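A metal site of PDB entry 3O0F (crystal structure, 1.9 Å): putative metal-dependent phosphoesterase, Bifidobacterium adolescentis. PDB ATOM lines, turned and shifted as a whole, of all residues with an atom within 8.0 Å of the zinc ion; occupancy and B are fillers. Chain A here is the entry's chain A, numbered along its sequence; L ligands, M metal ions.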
ATOM      1  N   HIS A  18     -10.208  20.720 -12.051  1.00  0.00           N
ATOM      2  CA  HIS A  18     -11.616  20.515 -12.359  1.00  0.00           C
ATOM      3  C   HIS A  18     -12.506  21.359 -11.428  1.00  0.00           C
ATOM      4  O   HIS A  18     -13.032  20.839 -10.432  1.00  0.00           O
ATOM      5  CB  HIS A  18     -11.910  19.039 -12.173  1.00  0.00           C
ATOM      6  CG  HIS A  18     -13.167  18.585 -12.831  1.00  0.00           C
ATOM      7  ND1 HIS A  18     -13.401  17.253 -13.140  1.00  0.00           N
ATOM      8  CD2 HIS A  18     -14.277  19.267 -13.200  1.00  0.00           C
ATOM      9  CE1 HIS A  18     -14.589  17.150 -13.709  1.00  0.00           C
ATOM     10  NE2 HIS A  18     -15.143  18.351 -13.753  1.00  0.00           N
ATOM     11  N   CYS A  19     -12.683  22.637 -11.749  1.00  0.00           N
ATOM     12  CA  CYS A  19     -13.388  23.594 -10.871  1.00  0.00           C
ATOM     13  C   CYS A  19     -14.366  24.427 -11.715  1.00  0.00           C
ATOM     14  O   CYS A  19     -13.989  24.894 -12.803  1.00  0.00           O
ATOM     15  CB  CYS A  19     -12.419  24.510 -10.153  1.00  0.00           C
ATOM     16  SG  CYS A  19     -11.103  23.664  -9.264  1.00  0.00           S
ATOM     17  N   HIS A  20     -15.606  24.557 -11.231  1.00  0.00           N
ATOM     18  CA  HIS A  20     -16.678  25.294 -11.879  1.00  0.00           C
ATOM     19  C   HIS A  20     -17.010  26.599 -11.142  1.00  0.00           C
ATOM     20  O   HIS A  20     -16.856  26.672  -9.917  1.00  0.00           O
ATOM     21  CB  HIS A  20     -17.924  24.421 -11.949  1.00  0.00           C
ATOM     22  CG  HIS A  20     -17.731  23.194 -12.774  1.00  0.00           C
ATOM     23  ND1 HIS A  20     -18.114  23.117 -14.081  1.00  0.00           N
ATOM     24  CD2 HIS A  20     -17.168  21.992 -12.476  1.00  0.00           C
ATOM     25  CE1 HIS A  20     -17.795  21.926 -14.564  1.00  0.00           C
ATOM     26  NE2 HIS A  20     -17.214  21.240 -13.623  1.00  0.00           N
ATOM     27  N   THR A  21     -17.514  27.595 -11.880  1.00  0.00           N
ATOM     28  CA  THR A  21     -17.791  28.910 -11.365  1.00  0.00           C
ATOM     29  C   THR A  21     -19.185  29.333 -11.782  1.00  0.00           C
ATOM     30  O   THR A  21     -19.896  28.596 -12.450  1.00  0.00           O
ATOM     31  CB  THR A  21     -16.748  29.958 -11.905  1.00  0.00           C
ATOM     32  OG1 THR A  21     -17.039  30.300 -13.270  1.00  0.00           O
ATOM     33  CG2 THR A  21     -15.288  29.419 -11.727  1.00  0.00           C
ATOM     34  N   SER A  24     -20.718  28.826 -15.271  1.00  0.00           N
ATOM     35  CA  SER A  24     -21.660  27.706 -15.525  1.00  0.00           C
ATOM     36  C   SER A  24     -22.499  27.403 -14.276  1.00  0.00           C
ATOM     37  O   SER A  24     -23.423  28.169 -13.961  1.00  0.00           O
ATOM     38  CB  SER A  24     -20.961  26.447 -16.103  1.00  0.00           C
ATOM     39  OG  SER A  24     -19.896  25.961 -15.310  1.00  0.00           O
ATOM     40  N   ASP A  25     -22.181  26.314 -13.571  1.00  0.00           N
ATOM     41  CA  ASP A  25     -23.003  25.876 -12.460  1.00  0.00           C
ATOM     42  C   ASP A  25     -22.362  25.953 -11.056  1.00  0.00           C
ATOM     43  O   ASP A  25     -22.900  25.396 -10.101  1.00  0.00           O
ATOM     44  CB  ASP A  25     -23.592  24.488 -12.725  1.00  0.00           C
ATOM     45  CG  ASP A  25     -22.548  23.396 -12.964  1.00  0.00           C
ATOM     46  OD1 ASP A  25     -21.321  23.679 -13.104  1.00  0.00           O
ATOM     47  OD2 ASP A  25     -22.985  22.200 -13.010  1.00  0.00           O
ATOM     48  N   GLY A  26     -21.201  26.620 -10.956  1.00  0.00           N
ATOM     49  CA  GLY A  26     -20.575  26.867  -9.674  1.00  0.00           C
ATOM     50  C   GLY A  26     -21.258  28.105  -9.061  1.00  0.00           C
ATOM     51  O   GLY A  26     -22.060  28.746  -9.706  1.00  0.00           O
ATOM     52  N   ALA A  48     -12.792  25.226 -15.422  1.00  0.00           N
ATOM     53  CA  ALA A  48     -13.283  24.181 -16.349  1.00  0.00           C
ATOM     54  C   ALA A  48     -14.778  24.252 -16.479  1.00  0.00           C
ATOM     55  O   ALA A  48     -15.462  23.220 -16.412  1.00  0.00           O
ATOM     56  CB  ALA A  48     -12.861  22.771 -15.865  1.00  0.00           C
ATOM     57  N   ASP A  49     -15.322  25.450 -16.652  1.00  0.00           N
ATOM     58  CA  ASP A  49     -16.764  25.554 -16.809  1.00  0.00           C
ATOM     59  C   ASP A  49     -17.335  24.803 -18.020  1.00  0.00           C
ATOM     60  O   ASP A  49     -16.645  24.574 -19.010  1.00  0.00           O
ATOM     61  CB  ASP A  49     -17.175  27.031 -16.875  1.00  0.00           C
ATOM     62  CG  ASP A  49     -17.050  27.730 -15.537  1.00  0.00           C
ATOM     63  OD1 ASP A  49     -17.691  27.244 -14.565  1.00  0.00           O
ATOM     64  OD2 ASP A  49     -16.311  28.743 -15.456  1.00  0.00           O
ATOM     65  N   HIS A  50     -18.614  24.451 -17.928  1.00  0.00           N
ATOM     66  CA  HIS A  50     -19.327  23.678 -18.966  1.00  0.00           C
ATOM     67  C   HIS A  50     -19.470  24.497 -20.245  1.00  0.00           C
ATOM     68  O   HIS A  50     -19.982  25.601 -20.203  1.00  0.00           O
ATOM     69  CB  HIS A  50     -20.731  23.328 -18.463  1.00  0.00           C
ATOM     70  CG  HIS A  50     -20.734  22.425 -17.288  1.00  0.00           C
ATOM     71  ND1 HIS A  50     -20.574  21.061 -17.405  1.00  0.00           N
ATOM     72  CD2 HIS A  50     -20.872  22.679 -15.961  1.00  0.00           C
ATOM     73  CE1 HIS A  50     -20.601  20.515 -16.206  1.00  0.00           C
ATOM     74  NE2 HIS A  50     -20.799  21.465 -15.322  1.00  0.00           N
ATOM     75  N   GLU A  75     -15.212  22.131 -19.568  1.00  0.00           N
ATOM     76  CA  GLU A  75     -15.768  20.776 -19.519  1.00  0.00           C
ATOM     77  C   GLU A  75     -16.819  20.691 -20.620  1.00  0.00           C
ATOM     78  O   GLU A  75     -17.816  21.404 -20.630  1.00  0.00           O
ATOM     79  CB  GLU A  75     -16.365  20.436 -18.144  1.00  0.00           C
ATOM     80  CG  GLU A  75     -16.917  19.057 -18.144  1.00  0.00           C
ATOM     81  CD  GLU A  75     -17.272  18.521 -16.752  1.00  0.00           C
ATOM     82  OE1 GLU A  75     -17.306  19.282 -15.835  1.00  0.00           O
ATOM     83  OE2 GLU A  75     -17.433  17.282 -16.599  1.00  0.00           O
ATOM     84  N   HIS A  86     -18.367  13.506 -20.267  1.00  0.00           N
ATOM     85  CA  HIS A  86     -17.840  14.836 -20.106  1.00  0.00           C
ATOM     86  C   HIS A  86     -16.336  14.799 -20.394  1.00  0.00           C
ATOM     87  O   HIS A  86     -15.614  13.923 -19.903  1.00  0.00           O
ATOM     88  CB  HIS A  86     -18.153  15.312 -18.672  1.00  0.00           C
ATOM     89  CG  HIS A  86     -19.600  15.659 -18.471  1.00  0.00           C
ATOM     90  ND1 HIS A  86     -20.057  16.366 -17.372  1.00  0.00           N
ATOM     91  CD2 HIS A  86     -20.695  15.440 -19.248  1.00  0.00           C
ATOM     92  CE1 HIS A  86     -21.362  16.537 -17.476  1.00  0.00           C
ATOM     93  NE2 HIS A  86     -21.771  15.990 -18.600  1.00  0.00           N
ATOM     94  N   ARG A 110     -28.789  23.639 -24.904  1.00  0.00           N
ATOM     95  CA  ARG A 110     -29.011  23.738 -23.428  1.00  0.00           C
ATOM     96  C   ARG A 110     -30.105  24.759 -22.990  1.00  0.00           C
ATOM     97  O   ARG A 110     -30.976  24.445 -22.193  1.00  0.00           O
ATOM     98  CB  ARG A 110     -27.725  24.113 -22.706  1.00  0.00           C
ATOM     99  CG  ARG A 110     -26.738  22.970 -22.526  1.00  0.00           C
ATOM    100  CD  ARG A 110     -25.466  23.475 -21.800  1.00  0.00           C
ATOM    101  NE  ARG A 110     -24.730  22.331 -21.245  1.00  0.00           N
ATOM    102  CZ  ARG A 110     -25.126  21.612 -20.185  1.00  0.00           C
ATOM    103  NH1 ARG A 110     -26.226  21.911 -19.526  1.00  0.00           N
ATOM    104  NH2 ARG A 110     -24.396  20.582 -19.782  1.00  0.00           N
ATOM    105  N   PRO A 147     -28.663  22.393 -12.992  1.00  0.00           N
ATOM    106  CA  PRO A 147     -28.371  22.997 -11.697  1.00  0.00           C
ATOM    107  C   PRO A 147     -29.077  24.304 -11.387  1.00  0.00           C
ATOM    108  O   PRO A 147     -29.398  24.538 -10.231  1.00  0.00           O
ATOM    109  CB  PRO A 147     -26.858  23.223 -11.746  1.00  0.00           C
ATOM    110  CG  PRO A 147     -26.372  22.128 -12.586  1.00  0.00           C
ATOM    111  CD  PRO A 147     -27.405  22.014 -13.686  1.00  0.00           C
ATOM    112  N   ARG A 162     -29.540  21.702  -3.414  1.00  0.00           N
ATOM    113  CA  ARG A 162     -29.524  21.430  -4.845  1.00  0.00           C
ATOM    114  C   ARG A 162     -29.472  19.940  -5.138  1.00  0.00           C
ATOM    115  O   ARG A 162     -30.177  19.450  -6.024  1.00  0.00           O
ATOM    116  CB  ARG A 162     -28.340  22.141  -5.483  1.00  0.00           C
ATOM    117  CG  ARG A 162     -28.304  22.085  -6.960  1.00  0.00           C
ATOM    118  CD  ARG A 162     -26.890  22.395  -7.449  1.00  0.00           C
ATOM    119  NE  ARG A 162     -26.600  23.815  -7.583  1.00  0.00           N
ATOM    120  CZ  ARG A 162     -25.530  24.279  -8.244  1.00  0.00           C
ATOM    121  NH1 ARG A 162     -24.665  23.436  -8.794  1.00  0.00           N
ATOM    122  NH2 ARG A 162     -25.335  25.575  -8.372  1.00  0.00           N
ATOM    123  N   HIS A 203     -14.241  11.889 -15.025  1.00  0.00           N
ATOM    124  CA  HIS A 203     -14.873  10.879 -14.117  1.00  0.00           C
ATOM    125  C   HIS A 203     -15.460   9.658 -14.891  1.00  0.00           C
ATOM    126  O   HIS A 203     -16.669   9.389 -14.829  1.00  0.00           O
ATOM    127  CB  HIS A 203     -15.946  11.581 -13.245  1.00  0.00           C
ATOM    128  CG  HIS A 203     -16.850  12.505 -14.009  1.00  0.00           C
ATOM    129  ND1 HIS A 203     -17.776  12.056 -14.932  1.00  0.00           N
ATOM    130  CD2 HIS A 203     -16.964  13.865 -14.000  1.00  0.00           C
ATOM    131  CE1 HIS A 203     -18.414  13.085 -15.472  1.00  0.00           C
ATOM    132  NE2 HIS A 203     -17.938  14.192 -14.923  1.00  0.00           N
ATOM    133  N   ASP A 261     -14.043  18.668  -8.891  1.00  0.00           N
ATOM    134  CA  ASP A 261     -15.363  19.004  -9.399  1.00  0.00           C
ATOM    135  C   ASP A 261     -16.057  19.991  -8.443  1.00  0.00           C
ATOM    136  O   ASP A 261     -17.249  19.910  -8.234  1.00  0.00           O
ATOM    137  CB  ASP A 261     -16.213  17.748  -9.556  1.00  0.00           C
ATOM    138  CG  ASP A 261     -16.905  17.695 -10.867  1.00  0.00           C
ATOM    139  OD1 ASP A 261     -17.155  18.772 -11.424  1.00  0.00           O
ATOM    140  OD2 ASP A 261     -17.146  16.569 -11.335  1.00  0.00           O
ATOM    141  N   TRP A 262     -15.290  20.905  -7.877  1.00  0.00           N
ATOM    142  CA  TRP A 262     -15.838  21.940  -7.041  1.00  0.00           C
ATOM    143  C   TRP A 262     -16.840  22.780  -7.805  1.00  0.00           C
ATOM    144  O   TRP A 262     -16.594  23.209  -8.946  1.00  0.00           O
ATOM    145  CB  TRP A 262     -14.704  22.809  -6.558  1.00  0.00           C
ATOM    146  CG  TRP A 262     -14.991  23.943  -5.638  1.00  0.00           C
ATOM    147  CD1 TRP A 262     -15.182  23.870  -4.309  1.00  0.00           C
ATOM    148  CD2 TRP A 262     -14.948  25.336  -5.975  1.00  0.00           C
ATOM    149  NE1 TRP A 262     -15.310  25.136  -3.777  1.00  0.00           N
ATOM    150  CE2 TRP A 262     -15.111  26.052  -4.779  1.00  0.00           C
ATOM    151  CE3 TRP A 262     -14.770  26.038  -7.178  1.00  0.00           C
ATOM    152  CZ2 TRP A 262     -15.161  27.431  -4.760  1.00  0.00           C
ATOM    153  CZ3 TRP A 262     -14.795  27.419  -7.157  1.00  0.00           C
ATOM    154  CH2 TRP A 262     -14.990  28.094  -5.944  1.00  0.00           C
ATOM    155  N   HIS A 263     -17.955  23.038  -7.132  1.00  0.00           N
ATOM    156  CA  HIS A 263     -18.962  23.955  -7.612  1.00  0.00           C
ATOM    157  C   HIS A 263     -19.311  24.931  -6.488  1.00  0.00           C
ATOM    158  O   HIS A 263     -20.425  25.465  -6.434  1.00  0.00           O
ATOM    159  CB  HIS A 263     -20.227  23.171  -7.995  1.00  0.00           C
ATOM    160  CG  HIS A 263     -20.114  22.344  -9.230  1.00  0.00           C
ATOM    161  ND1 HIS A 263     -19.271  21.251  -9.356  1.00  0.00           N
ATOM    162  CD2 HIS A 263     -20.785  22.419 -10.400  1.00  0.00           C
ATOM    163  CE1 HIS A 263     -19.428  20.710 -10.544  1.00  0.00           C
ATOM    164  NE2 HIS A 263     -20.350  21.396 -11.192  1.00  0.00           N
ATOM    165  N   LYS A 267     -22.324  21.912  -4.539  1.00  0.00           N
ATOM    166  CA  LYS A 267     -22.079  20.504  -4.307  1.00  0.00           C
ATOM    167  C   LYS A 267     -21.299  20.364  -3.013  1.00  0.00           C
ATOM    168  O   LYS A 267     -20.687  21.299  -2.565  1.00  0.00           O
ATOM    169  CB  LYS A 267     -21.236  19.912  -5.454  1.00  0.00           C
ATOM    170  CG  LYS A 267     -21.962  19.544  -6.742  1.00  0.00           C
ATOM    171  CD  LYS A 267     -21.023  18.746  -7.632  1.00  0.00           C
ATOM    172  CE  LYS A 267     -21.593  18.364  -8.985  1.00  0.00           C
ATOM    173  NZ  LYS A 267     -20.567  17.542  -9.683  1.00  0.00           N
HETATM  174  P1  LIG L   1     -20.522  18.408 -13.310  1.00  0.00           P
HETATM  175  O1  LIG L   1     -20.756  17.517 -12.103  1.00  0.00           O
HETATM  176  O2  LIG L   1     -20.635  17.530 -14.537  1.00  0.00           O
HETATM  177  O3  LIG L   1     -21.378  19.698 -13.282  1.00  0.00           O
HETATM  178  O4  LIG L   1     -19.185  19.053 -13.285  1.00  0.00           O
HETATM  179  P1  LG2 L   2     -27.330  19.043 -17.325  1.00  0.00           P
HETATM  180  O1  LG2 L   2     -26.033  18.967 -18.064  1.00  0.00           O
HETATM  181  O2  LG2 L   2     -27.994  20.367 -17.605  1.00  0.00           O
HETATM  182  O3  LG2 L   2     -28.242  17.829 -17.512  1.00  0.00           O
HETATM  183  O4  LG2 L   2     -26.951  19.074 -15.768  1.00  0.00           O
HETATM  184  C1  LG2 L   2     -26.378  17.942 -15.153  1.00  0.00           C
HETATM  185  C2  LG2 L   2     -25.180  18.422 -14.391  1.00  0.00           C
HETATM  186  O5  LG2 L   2     -25.538  19.055 -13.137  1.00  0.00           O
HETATM  187  C3  LG2 L   2     -24.248  17.261 -14.070  1.00  0.00           C
HETATM  188  O6  LG2 L   2     -23.094  17.350 -14.895  1.00  0.00           O
HETATM  189  C4  LG2 L   2     -23.900  17.621 -12.636  1.00  0.00           C
HETATM  190  O7  LG2 L   2     -22.984  16.895 -11.822  1.00  0.00           O
HETATM  191  C5  LG2 L   2     -24.341  19.060 -12.372  1.00  0.00           C
HETATM  192  N1  LG2 L   2     -24.542  19.346 -10.937  1.00  0.00           N
HETATM  193  C6  LG2 L   2     -24.189  20.480 -10.336  1.00  0.00           C
HETATM  194  N2  LG2 L   2     -24.523  20.433  -9.026  1.00  0.00           N
HETATM  195  C7  LG2 L   2     -25.096  19.246  -8.781  1.00  0.00           C
HETATM  196  C8  LG2 L   2     -25.663  18.557  -7.607  1.00  0.00           C
HETATM  197  N3  LG2 L   2     -25.683  19.158  -6.370  1.00  0.00           N
HETATM  198  N4  LG2 L   2     -26.177  17.335  -7.812  1.00  0.00           N
HETATM  199  C9  LG2 L   2     -26.182  16.712  -9.011  1.00  0.00           C
HETATM  200  N5  LG2 L   2     -25.674  17.275 -10.111  1.00  0.00           N
HETATM  201  C10 LG2 L   2     -25.118  18.522 -10.050  1.00  0.00           C
HETATM  202 ZN    ZN M   1     -20.898  21.385 -13.198  1.00  0.00          ZN
HETATM  203 FE    FE M   2     -17.274  18.943 -13.701  1.00  0.00          FE
HETATM  204 FE    FE M   3     -18.808  16.283 -15.292  1.00  0.00          FE
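The guanidinium group (NH2) of Arg 110 lies within salt-bridge range of an oxygen (O1) of LG2 L2, at 2.9 Å. NH1 of Arg 162 lies within hydrogen-bond range of N2 of LG2 L2 (3.0 Å). The side-chain amino group of Lys 267 lies within hydrogen-bond range of an oxygen (O7) of LG2 L2, at 3.3 Å.
A ring nitrogen (ND1) of His 263 is in hydrogen-bond range of the backbone carbonyl oxygen (O) of Asp 261, at 2.7 Å. The backbone NH of His 20 lies within hydrogen-bond range of the backbone carbonyl oxygen of Trp 262, 2.8 Å away. A ring nitrogen (ND1) of His 20 lies close to the side-chain carboxylate (OD1) of Asp 25 (3.4 Å). OD1 of Asp 25 lies close to OG of Ser 24 (3.5 Å). A ring nitrogen (NE2) of His 50 sits close to a ring nitrogen (ND1) of His 20, at 3.4 Å. The backbone NH (N) of His 50 lies within hydrogen-bond range of the side-chain hydroxyl (OG) of Ser 24, at 3.3 Å. The guanidinium group of Arg 162 is in hydrogen-bond range of the backbone carbonyl oxygen of Asp 25 (2.9 Å).
His 20 touches the zinc ion. Four residues have an atom within 4 Å of the zinc ion: His 20, Asp 25, His 50 and His 263.
O3 of LIG L1 binds the zinc ion, at 1.8 Å. A ring nitrogen (NE2) of His 263 binds the zinc ion, 2.1 Å away. A ring nitrogen (NE2) of His 50 is bound to the zinc ion. The zinc ion is bound by OD2 of Asp 25, at 2.2 Å. The zinc ion is bound by OD1 of Asp 25 (2.3 Å).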
